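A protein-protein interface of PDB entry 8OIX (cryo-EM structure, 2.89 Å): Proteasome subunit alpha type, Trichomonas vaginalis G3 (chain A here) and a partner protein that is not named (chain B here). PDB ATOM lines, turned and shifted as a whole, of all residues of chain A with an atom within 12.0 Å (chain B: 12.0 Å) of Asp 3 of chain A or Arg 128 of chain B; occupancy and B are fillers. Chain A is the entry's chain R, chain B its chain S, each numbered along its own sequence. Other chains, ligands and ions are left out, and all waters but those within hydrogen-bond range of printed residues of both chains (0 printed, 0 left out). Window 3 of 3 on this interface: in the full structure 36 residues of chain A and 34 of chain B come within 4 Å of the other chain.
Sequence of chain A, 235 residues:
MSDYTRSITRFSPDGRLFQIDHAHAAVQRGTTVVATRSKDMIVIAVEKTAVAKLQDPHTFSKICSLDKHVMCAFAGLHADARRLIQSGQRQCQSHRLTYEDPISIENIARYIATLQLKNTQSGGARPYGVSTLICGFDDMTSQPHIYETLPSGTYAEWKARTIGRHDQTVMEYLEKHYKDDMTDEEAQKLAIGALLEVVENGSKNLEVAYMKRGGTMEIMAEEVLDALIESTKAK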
ATOM      1  N   ASP A   3      12.303  36.872 -16.885  1.00  0.00           N
ATOM      2  CA  ASP A   3      11.736  36.150 -15.752  1.00  0.00           C
ATOM      3  C   ASP A   3      12.795  35.260 -15.103  1.00  0.00           C
ATOM      4  O   ASP A   3      13.918  35.152 -15.595  1.00  0.00           O
ATOM      5  CB  ASP A   3      10.528  35.320 -16.193  1.00  0.00           C
ATOM      6  CG  ASP A   3       9.571  35.026 -15.051  1.00  0.00           C
ATOM      7  OD1 ASP A   3      10.035  34.898 -13.898  1.00  0.00           O
ATOM      8  OD2 ASP A   3       8.352  34.926 -15.305  1.00  0.00           O
ATOM      9  N   TYR A   4      12.424  34.632 -13.992  1.00  0.00           N
ATOM     10  CA  TYR A   4      13.350  33.798 -13.238  1.00  0.00           C
ATOM     11  C   TYR A   4      13.685  32.529 -14.012  1.00  0.00           C
ATOM     12  O   TYR A   4      12.789  31.812 -14.469  1.00  0.00           O
ATOM     13  CB  TYR A   4      12.715  33.458 -11.892  1.00  0.00           C
ATOM     14  CG  TYR A   4      13.502  32.566 -10.962  1.00  0.00           C
ATOM     15  CD1 TYR A   4      14.488  33.085 -10.140  1.00  0.00           C
ATOM     16  CD2 TYR A   4      13.214  31.214 -10.863  1.00  0.00           C
ATOM     17  CE1 TYR A   4      15.189  32.276  -9.273  1.00  0.00           C
ATOM     18  CE2 TYR A   4      13.910  30.396  -9.998  1.00  0.00           C
ATOM     19  CZ  TYR A   4      14.889  30.936  -9.199  1.00  0.00           C
ATOM     20  OH  TYR A   4      15.588  30.131  -8.329  1.00  0.00           O
ATOM     21  N   THR A   5      14.989  32.249 -14.155  1.00  0.00           N
ATOM     22  CA  THR A   5      15.510  31.071 -14.852  1.00  0.00           C
ATOM     23  C   THR A   5      16.765  30.598 -14.115  1.00  0.00           C
ATOM     24  O   THR A   5      17.897  30.910 -14.476  1.00  0.00           O
ATOM     25  CB  THR A   5      15.829  31.359 -16.321  1.00  0.00           C
ATOM     26  OG1 THR A   5      16.712  32.483 -16.411  1.00  0.00           O
ATOM     27  CG2 THR A   5      14.567  31.636 -17.118  1.00  0.00           C
ATOM     28  N   ARG A   6      16.576  29.816 -13.053  1.00  0.00           N
ATOM     29  CA  ARG A   6      17.690  29.358 -12.234  1.00  0.00           C
ATOM     30  C   ARG A   6      18.049  27.904 -12.522  1.00  0.00           C
ATOM     31  O   ARG A   6      18.840  27.309 -11.785  1.00  0.00           O
ATOM     32  CB  ARG A   6      17.348  29.561 -10.754  1.00  0.00           C
ATOM     33  CG  ARG A   6      18.425  29.242  -9.711  1.00  0.00           C
ATOM     34  CD  ARG A   6      18.054  28.000  -8.908  1.00  0.00           C
ATOM     35  NE  ARG A   6      18.963  27.754  -7.795  1.00  0.00           N
ATOM     36  CZ  ARG A   6      18.862  26.728  -6.961  1.00  0.00           C
ATOM     37  NH1 ARG A   6      17.930  25.801  -7.117  1.00  0.00           N
ATOM     38  NH2 ARG A   6      19.725  26.621  -5.955  1.00  0.00           N
ATOM     39  N   SER A   7      17.557  27.352 -13.626  1.00  0.00           N
ATOM     40  CA  SER A   7      17.864  25.982 -14.032  1.00  0.00           C
ATOM     41  C   SER A   7      17.832  25.051 -12.824  1.00  0.00           C
ATOM     42  O   SER A   7      18.843  24.488 -12.407  1.00  0.00           O
ATOM     43  CB  SER A   7      19.210  25.907 -14.742  1.00  0.00           C
ATOM     44  OG  SER A   7      19.466  24.586 -15.181  1.00  0.00           O
ATOM     45  N   ILE A   8      16.645  24.949 -12.224  1.00  0.00           N
ATOM     46  CA  ILE A   8      16.469  24.118 -11.035  1.00  0.00           C
ATOM     47  C   ILE A   8      16.985  22.708 -11.283  1.00  0.00           C
ATOM     48  O   ILE A   8      17.661  22.117 -10.432  1.00  0.00           O
ATOM     49  CB  ILE A   8      14.991  24.118 -10.593  1.00  0.00           C
ATOM     50  CG1 ILE A   8      14.656  25.373  -9.777  1.00  0.00           C
ATOM     51  CG2 ILE A   8      14.659  22.872  -9.800  1.00  0.00           C
ATOM     52  CD1 ILE A   8      14.635  26.660 -10.560  1.00  0.00           C
ATOM     53  N   ARG A  83      -2.140  20.956 -11.303  1.00  0.00           N
ATOM     54  CA  ARG A  83      -1.673  21.668 -12.489  1.00  0.00           C
ATOM     55  C   ARG A  83      -1.558  20.730 -13.685  1.00  0.00           C
ATOM     56  O   ARG A  83      -1.954  21.086 -14.803  1.00  0.00           O
ATOM     57  CB  ARG A  83      -0.336  22.353 -12.209  1.00  0.00           C
ATOM     58  CG  ARG A  83      -0.058  23.514 -13.144  1.00  0.00           C
ATOM     59  CD  ARG A  83       1.316  24.113 -12.923  1.00  0.00           C
ATOM     60  NE  ARG A  83       1.532  25.280 -13.770  1.00  0.00           N
ATOM     61  CZ  ARG A  83       1.142  26.511 -13.465  1.00  0.00           C
ATOM     62  NH1 ARG A  83       0.508  26.775 -12.334  1.00  0.00           N
ATOM     63  NH2 ARG A  83       1.393  27.501 -14.316  1.00  0.00           N
ATOM     64  N   GLN A 121      13.146  20.860 -17.897  1.00  0.00           N
ATOM     65  CA  GLN A 121      14.000  21.556 -18.850  1.00  0.00           C
ATOM     66  C   GLN A 121      13.902  23.069 -18.771  1.00  0.00           C
ATOM     67  O   GLN A 121      14.858  23.751 -19.134  1.00  0.00           O
ATOM     68  CB  GLN A 121      13.669  21.121 -20.283  1.00  0.00           C
ATOM     69  CG  GLN A 121      13.996  19.673 -20.597  1.00  0.00           C
ATOM     70  CD  GLN A 121      13.550  19.267 -21.989  1.00  0.00           C
ATOM     71  OE1 GLN A 121      12.690  19.910 -22.591  1.00  0.00           O
ATOM     72  NE2 GLN A 121      14.143  18.202 -22.513  1.00  0.00           N
ATOM     73  N   SER A 122      12.769  23.608 -18.330  1.00  0.00           N
ATOM     74  CA  SER A 122      12.591  25.051 -18.293  1.00  0.00           C
ATOM     75  C   SER A 122      13.271  25.621 -17.056  1.00  0.00           C
ATOM     76  O   SER A 122      13.073  25.124 -15.943  1.00  0.00           O
ATOM     77  CB  SER A 122      11.106  25.412 -18.293  1.00  0.00           C
ATOM     78  OG  SER A 122      10.466  24.931 -19.461  1.00  0.00           O
ATOM     79  N   GLY A 123      14.081  26.656 -17.253  1.00  0.00           N
ATOM     80  CA  GLY A 123      14.691  27.326 -16.125  1.00  0.00           C
ATOM     81  C   GLY A 123      13.653  28.013 -15.259  1.00  0.00           C
ATOM     82  O   GLY A 123      12.645  28.528 -15.741  1.00  0.00           O
ATOM     83  N   GLY A 124      13.908  28.014 -13.955  1.00  0.00           N
ATOM     84  CA  GLY A 124      12.951  28.583 -13.029  1.00  0.00           C
ATOM     85  C   GLY A 124      11.677  27.789 -12.879  1.00  0.00           C
ATOM     86  O   GLY A 124      10.669  28.333 -12.422  1.00  0.00           O
ATOM     87  N   ALA A 125      11.689  26.511 -13.252  1.00  0.00           N
ATOM     88  CA  ALA A 125      10.513  25.655 -13.175  1.00  0.00           C
ATOM     89  C   ALA A 125      10.864  24.400 -12.392  1.00  0.00           C
ATOM     90  O   ALA A 125      11.828  23.705 -12.728  1.00  0.00           O
ATOM     91  CB  ALA A 125      10.002  25.292 -14.571  1.00  0.00           C
ATOM     92  N   ARG A 126      10.082  24.115 -11.353  1.00  0.00           N
ATOM     93  CA  ARG A 126      10.331  22.970 -10.489  1.00  0.00           C
ATOM     94  C   ARG A 126       9.683  21.728 -11.083  1.00  0.00           C
ATOM     95  O   ARG A 126       8.483  21.762 -11.389  1.00  0.00           O
ATOM     96  CB  ARG A 126       9.773  23.207  -9.099  1.00  0.00           C
ATOM     97  CG  ARG A 126      10.208  22.156  -8.093  1.00  0.00           C
ATOM     98  CD  ARG A 126       9.601  22.386  -6.718  1.00  0.00           C
ATOM     99  NE  ARG A 126       8.199  22.794  -6.749  1.00  0.00           N
ATOM    100  CZ  ARG A 126       7.199  22.053  -7.210  1.00  0.00           C
ATOM    101  NH1 ARG A 126       7.396  20.828  -7.666  1.00  0.00           N
ATOM    102  NH2 ARG A 126       5.964  22.545  -7.188  1.00  0.00           N
ATOM    103  N   VAL B  12      24.991  26.131 -15.033  1.00  0.00           N
ATOM    104  CA  VAL B  12      24.983  25.046 -16.013  1.00  0.00           C
ATOM    105  C   VAL B  12      26.057  25.263 -17.074  1.00  0.00           C
ATOM    106  O   VAL B  12      26.771  24.328 -17.458  1.00  0.00           O
ATOM    107  CB  VAL B  12      23.586  24.886 -16.641  1.00  0.00           C
ATOM    108  CG1 VAL B  12      22.593  24.433 -15.597  1.00  0.00           C
ATOM    109  CG2 VAL B  12      23.122  26.171 -17.295  1.00  0.00           C
ATOM    110  N   ASN B  13      26.190  26.491 -17.563  1.00  0.00           N
ATOM    111  CA  ASN B  13      27.118  26.787 -18.650  1.00  0.00           C
ATOM    112  C   ASN B  13      28.444  27.294 -18.083  1.00  0.00           C
ATOM    113  O   ASN B  13      28.856  28.437 -18.278  1.00  0.00           O
ATOM    114  CB  ASN B  13      26.488  27.780 -19.623  1.00  0.00           C
ATOM    115  CG  ASN B  13      25.838  28.958 -18.922  1.00  0.00           C
ATOM    116  OD1 ASN B  13      26.267  29.375 -17.845  1.00  0.00           O
ATOM    117  ND2 ASN B  13      24.788  29.498 -19.529  1.00  0.00           N
ATOM    118  N   ALA B 122      21.865  24.410 -26.880  1.00  0.00           N
ATOM    119  CA  ALA B 122      21.227  25.702 -26.675  1.00  0.00           C
ATOM    120  C   ALA B 122      20.701  25.884 -25.257  1.00  0.00           C
ATOM    121  O   ALA B 122      19.810  26.711 -25.041  1.00  0.00           O
ATOM    122  CB  ALA B 122      20.092  25.894 -27.683  1.00  0.00           C
ATOM    123  N   PHE B 123      21.224  25.132 -24.292  1.00  0.00           N
ATOM    124  CA  PHE B 123      20.779  25.253 -22.912  1.00  0.00           C
ATOM    125  C   PHE B 123      21.410  26.465 -22.239  1.00  0.00           C
ATOM    126  O   PHE B 123      22.552  26.837 -22.520  1.00  0.00           O
ATOM    127  CB  PHE B 123      21.100  23.979 -22.129  1.00  0.00           C
ATOM    128  CG  PHE B 123      22.562  23.784 -21.841  1.00  0.00           C
ATOM    129  CD1 PHE B 123      23.380  23.139 -22.752  1.00  0.00           C
ATOM    130  CD2 PHE B 123      23.114  24.218 -20.646  1.00  0.00           C
ATOM    131  CE1 PHE B 123      24.721  22.951 -22.487  1.00  0.00           C
ATOM    132  CE2 PHE B 123      24.453  24.032 -20.377  1.00  0.00           C
ATOM    133  CZ  PHE B 123      25.258  23.397 -21.298  1.00  0.00           C
ATOM    134  N   GLY B 124      20.648  27.081 -21.339  1.00  0.00           N
ATOM    135  CA  GLY B 124      21.116  28.274 -20.665  1.00  0.00           C
ATOM    136  C   GLY B 124      20.390  28.516 -19.364  1.00  0.00           C
ATOM    137  O   GLY B 124      19.297  27.995 -19.124  1.00  0.00           O
ATOM    138  N   GLU B 125      21.027  29.323 -18.520  1.00  0.00           N
ATOM    139  CA  GLU B 125      20.531  29.674 -17.198  1.00  0.00           C
ATOM    140  C   GLU B 125      20.955  31.106 -16.919  1.00  0.00           C
ATOM    141  O   GLU B 125      21.939  31.589 -17.478  1.00  0.00           O
ATOM    142  CB  GLU B 125      21.090  28.719 -16.135  1.00  0.00           C
ATOM    143  CG  GLU B 125      20.921  29.141 -14.687  1.00  0.00           C
ATOM    144  CD  GLU B 125      21.665  28.224 -13.738  1.00  0.00           C
ATOM    145  OE1 GLU B 125      22.680  27.634 -14.160  1.00  0.00           O
ATOM    146  OE2 GLU B 125      21.254  28.108 -12.566  1.00  0.00           O
ATOM    147  N   GLY B 126      20.197  31.795 -16.068  1.00  0.00           N
ATOM    148  CA  GLY B 126      20.595  33.106 -15.603  1.00  0.00           C
ATOM    149  C   GLY B 126      20.131  34.269 -16.450  1.00  0.00           C
ATOM    150  O   GLY B 126      20.321  35.422 -16.044  1.00  0.00           O
ATOM    151  N   ARG B 127      19.561  34.015 -17.624  1.00  0.00           N
ATOM    152  CA  ARG B 127      19.052  35.066 -18.491  1.00  0.00           C
ATOM    153  C   ARG B 127      17.531  35.032 -18.511  1.00  0.00           C
ATOM    154  O   ARG B 127      16.925  33.956 -18.486  1.00  0.00           O
ATOM    155  CB  ARG B 127      19.597  34.926 -19.914  1.00  0.00           C
ATOM    156  CG  ARG B 127      20.758  35.858 -20.237  1.00  0.00           C
ATOM    157  CD  ARG B 127      20.385  37.330 -20.076  1.00  0.00           C
ATOM    158  NE  ARG B 127      19.001  37.611 -20.447  1.00  0.00           N
ATOM    159  CZ  ARG B 127      18.569  37.750 -21.693  1.00  0.00           C
ATOM    160  NH1 ARG B 127      19.384  37.625 -22.727  1.00  0.00           N
ATOM    161  NH2 ARG B 127      17.283  38.018 -21.906  1.00  0.00           N
ATOM    162  N   ARG B 128      16.924  36.215 -18.551  1.00  0.00           N
ATOM    163  CA  ARG B 128      15.471  36.316 -18.573  1.00  0.00           C
ATOM    164  C   ARG B 128      14.903  35.624 -19.806  1.00  0.00           C
ATOM    165  O   ARG B 128      15.509  35.637 -20.880  1.00  0.00           O
ATOM    166  CB  ARG B 128      15.047  37.785 -18.549  1.00  0.00           C
ATOM    167  CG  ARG B 128      15.757  38.619 -17.495  1.00  0.00           C
ATOM    168  CD  ARG B 128      15.568  38.033 -16.106  1.00  0.00           C
ATOM    169  NE  ARG B 128      14.922  38.974 -15.198  1.00  0.00           N
ATOM    170  CZ  ARG B 128      15.568  39.883 -14.480  1.00  0.00           C
ATOM    171  NH1 ARG B 128      16.882  40.013 -14.549  1.00  0.00           N
ATOM    172  NH2 ARG B 128      14.875  40.683 -13.674  1.00  0.00           N
ATOM    173  N   LYS B 129      13.740  34.999 -19.636  1.00  0.00           N
ATOM    174  CA  LYS B 129      13.089  34.236 -20.699  1.00  0.00           C
ATOM    175  C   LYS B 129      12.917  35.050 -21.978  1.00  0.00           C
ATOM    176  O   LYS B 129      12.415  36.175 -21.947  1.00  0.00           O
ATOM    177  CB  LYS B 129      11.728  33.724 -20.224  1.00  0.00           C
ATOM    178  CG  LYS B 129      11.797  32.841 -18.994  1.00  0.00           C
ATOM    179  CD  LYS B 129      10.416  32.415 -18.530  1.00  0.00           C
ATOM    180  CE  LYS B 129      10.474  31.780 -17.150  1.00  0.00           C
ATOM    181  NZ  LYS B 129       9.115  31.537 -16.595  1.00  0.00           N
ATOM    182  N   GLN B 134      13.718  28.620 -23.450  1.00  0.00           N
ATOM    183  CA  GLN B 134      15.022  27.979 -23.555  1.00  0.00           C
ATOM    184  C   GLN B 134      15.169  26.846 -22.546  1.00  0.00           C
ATOM    185  O   GLN B 134      14.705  26.947 -21.411  1.00  0.00           O
ATOM    186  CB  GLN B 134      16.141  29.003 -23.348  1.00  0.00           C
ATOM    187  CG  GLN B 134      17.532  28.461 -23.628  1.00  0.00           C
ATOM    188  CD  GLN B 134      18.631  29.390 -23.153  1.00  0.00           C
ATOM    189  OE1 GLN B 134      18.529  29.997 -22.088  1.00  0.00           O
ATOM    190  NE2 GLN B 134      19.692  29.501 -23.943  1.00  0.00           N
ATOM    191  N   MET B 135      15.816  25.765 -22.971  1.00  0.00           N
ATOM    192  CA  MET B 135      16.110  24.662 -22.069  1.00  0.00           C
ATOM    193  C   MET B 135      17.182  25.070 -21.064  1.00  0.00           C
ATOM    194  O   MET B 135      18.058  25.888 -21.350  1.00  0.00           O
ATOM    195  CB  MET B 135      16.550  23.437 -22.872  1.00  0.00           C
ATOM    196  CG  MET B 135      17.733  23.707 -23.784  1.00  0.00           C
ATOM    197  SD  MET B 135      17.946  22.497 -25.104  1.00  0.00           S
ATOM    198  CE  MET B 135      18.822  21.196 -24.249  1.00  0.00           C
ATOM    199  N   SER B 136      17.095  24.500 -19.862  1.00  0.00           N
ATOM    200  CA  SER B 136      17.960  24.889 -18.757  1.00  0.00           C
ATOM    201  C   SER B 136      19.156  23.968 -18.567  1.00  0.00           C
ATOM    202  O   SER B 136      20.028  24.275 -17.748  1.00  0.00           O
ATOM    203  CB  SER B 136      17.158  24.946 -17.452  1.00  0.00           C
ATOM    204  OG  SER B 136      16.734  23.655 -17.055  1.00  0.00           O
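Arg 128 of chain B touches Asp 3 of chain A (CB to N, 3.3 Å).
Tyr 4 of chain A touches Lys 129 of chain B (O to CE, 3.5 Å).
O of Thr 5 of chain A touches CG of Glu 125 of chain B, at 3.5 Å.
Lys 129 of chain B touches Thr 5 of chain A.
OG of Ser 7 of chain A touches CG1 of Val 12 of chain B (3.2 Å).
Glu 125 of chain B touches Ser 7 of chain A.
O of Gln 134 of chain B touches O of Gln 121 of chain A (3.9 Å).
C of Met 135 of chain B touches O of Gln 121 of chain A, at 3.3 Å.
C of Ser 122 of chain A touches CB of Ser 136 of chain B, at 3.96 Å.
N of Gly 123 of chain A touches CB of Ser 136 of chain B, 3.5 Å away.
Of the 13 printed residues of chain A, 8 touch a printed residue of chain B.
Of the 13 printed residues of chain B, 9 touch a printed residue of chain A.
Arg 128 of chain B touches just one residue of chain A: Asp 3.
Thr 5 of chain A touches four residues of chain B.
No residue of chain B comes within 4 Å of Gly 124 of chain A.
Of chain A, only Thr 5 comes within 4 Å of Gly 126 of chain B.
Printed residues of chain A within 4 Å of Arg 127 of chain B: Thr 5 (2.6 Å).
Of the printed residues of chain A, Val 12 of chain B touches Ser 7 (3.2 Å).
Of the printed residues of chain A, Met 135 of chain B touches Gln 121 (3.3 Å).
Of the printed residues of chain B, Arg 6 of chain A touches Glu 125.
Of the printed residues of chain B, Ser 7 of chain A touches Val 12 (3.2 Å), Glu 125 (3.5 Å) and Ser 136 (2.6 Å).
Asn 13 of chain B touches none of the printed residues of chain A.
The nearest residue of chain B that does not touch Asp 3 of chain A is Arg 127 of chain B (4.3 Å).
The backbone carbonyl oxygen of Gln 121 of chain A is in hydrogen-bond range of the backbone NH of Ser 136 of chain B.
O of Thr 5 of chain A sits at hydrogen-bond distance from N of Gly 126 of chain B (2.9 Å).
The side-chain hydroxyl (OG) of Ser 7 of chain A sits at hydrogen-bond distance from the backbone carbonyl oxygen (O) of Ser 136 of chain B (2.6 Å).
The side-chain carboxylate of Asp 3 of chain A lies within salt-bridge range of the side-chain amino group of Lys 129 of chain B (3.7 Å).
The backbone carbonyl oxygen (O) of Arg 6 of chain A lies close to the side-chain carboxylate (OE2) of Glu 125 of chain B (2.7 Å).
The side-chain hydroxyl (OG1) of Thr 5 of chain A sits at hydrogen-bond distance from the backbone carbonyl oxygen (O) of Arg 127 of chain B.
NE2 of Gln 134 of chain B is in hydrogen-bond range of O of Ala 122 of chain B, at 3.0 Å.
N of Val 12 of chain B is in hydrogen-bond range of OE1 of Glu 125 of chain B, 2.9 Å away.
N of Gly 124 of chain B lies within hydrogen-bond range of O of Met 135 of chain B (2.9 Å).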
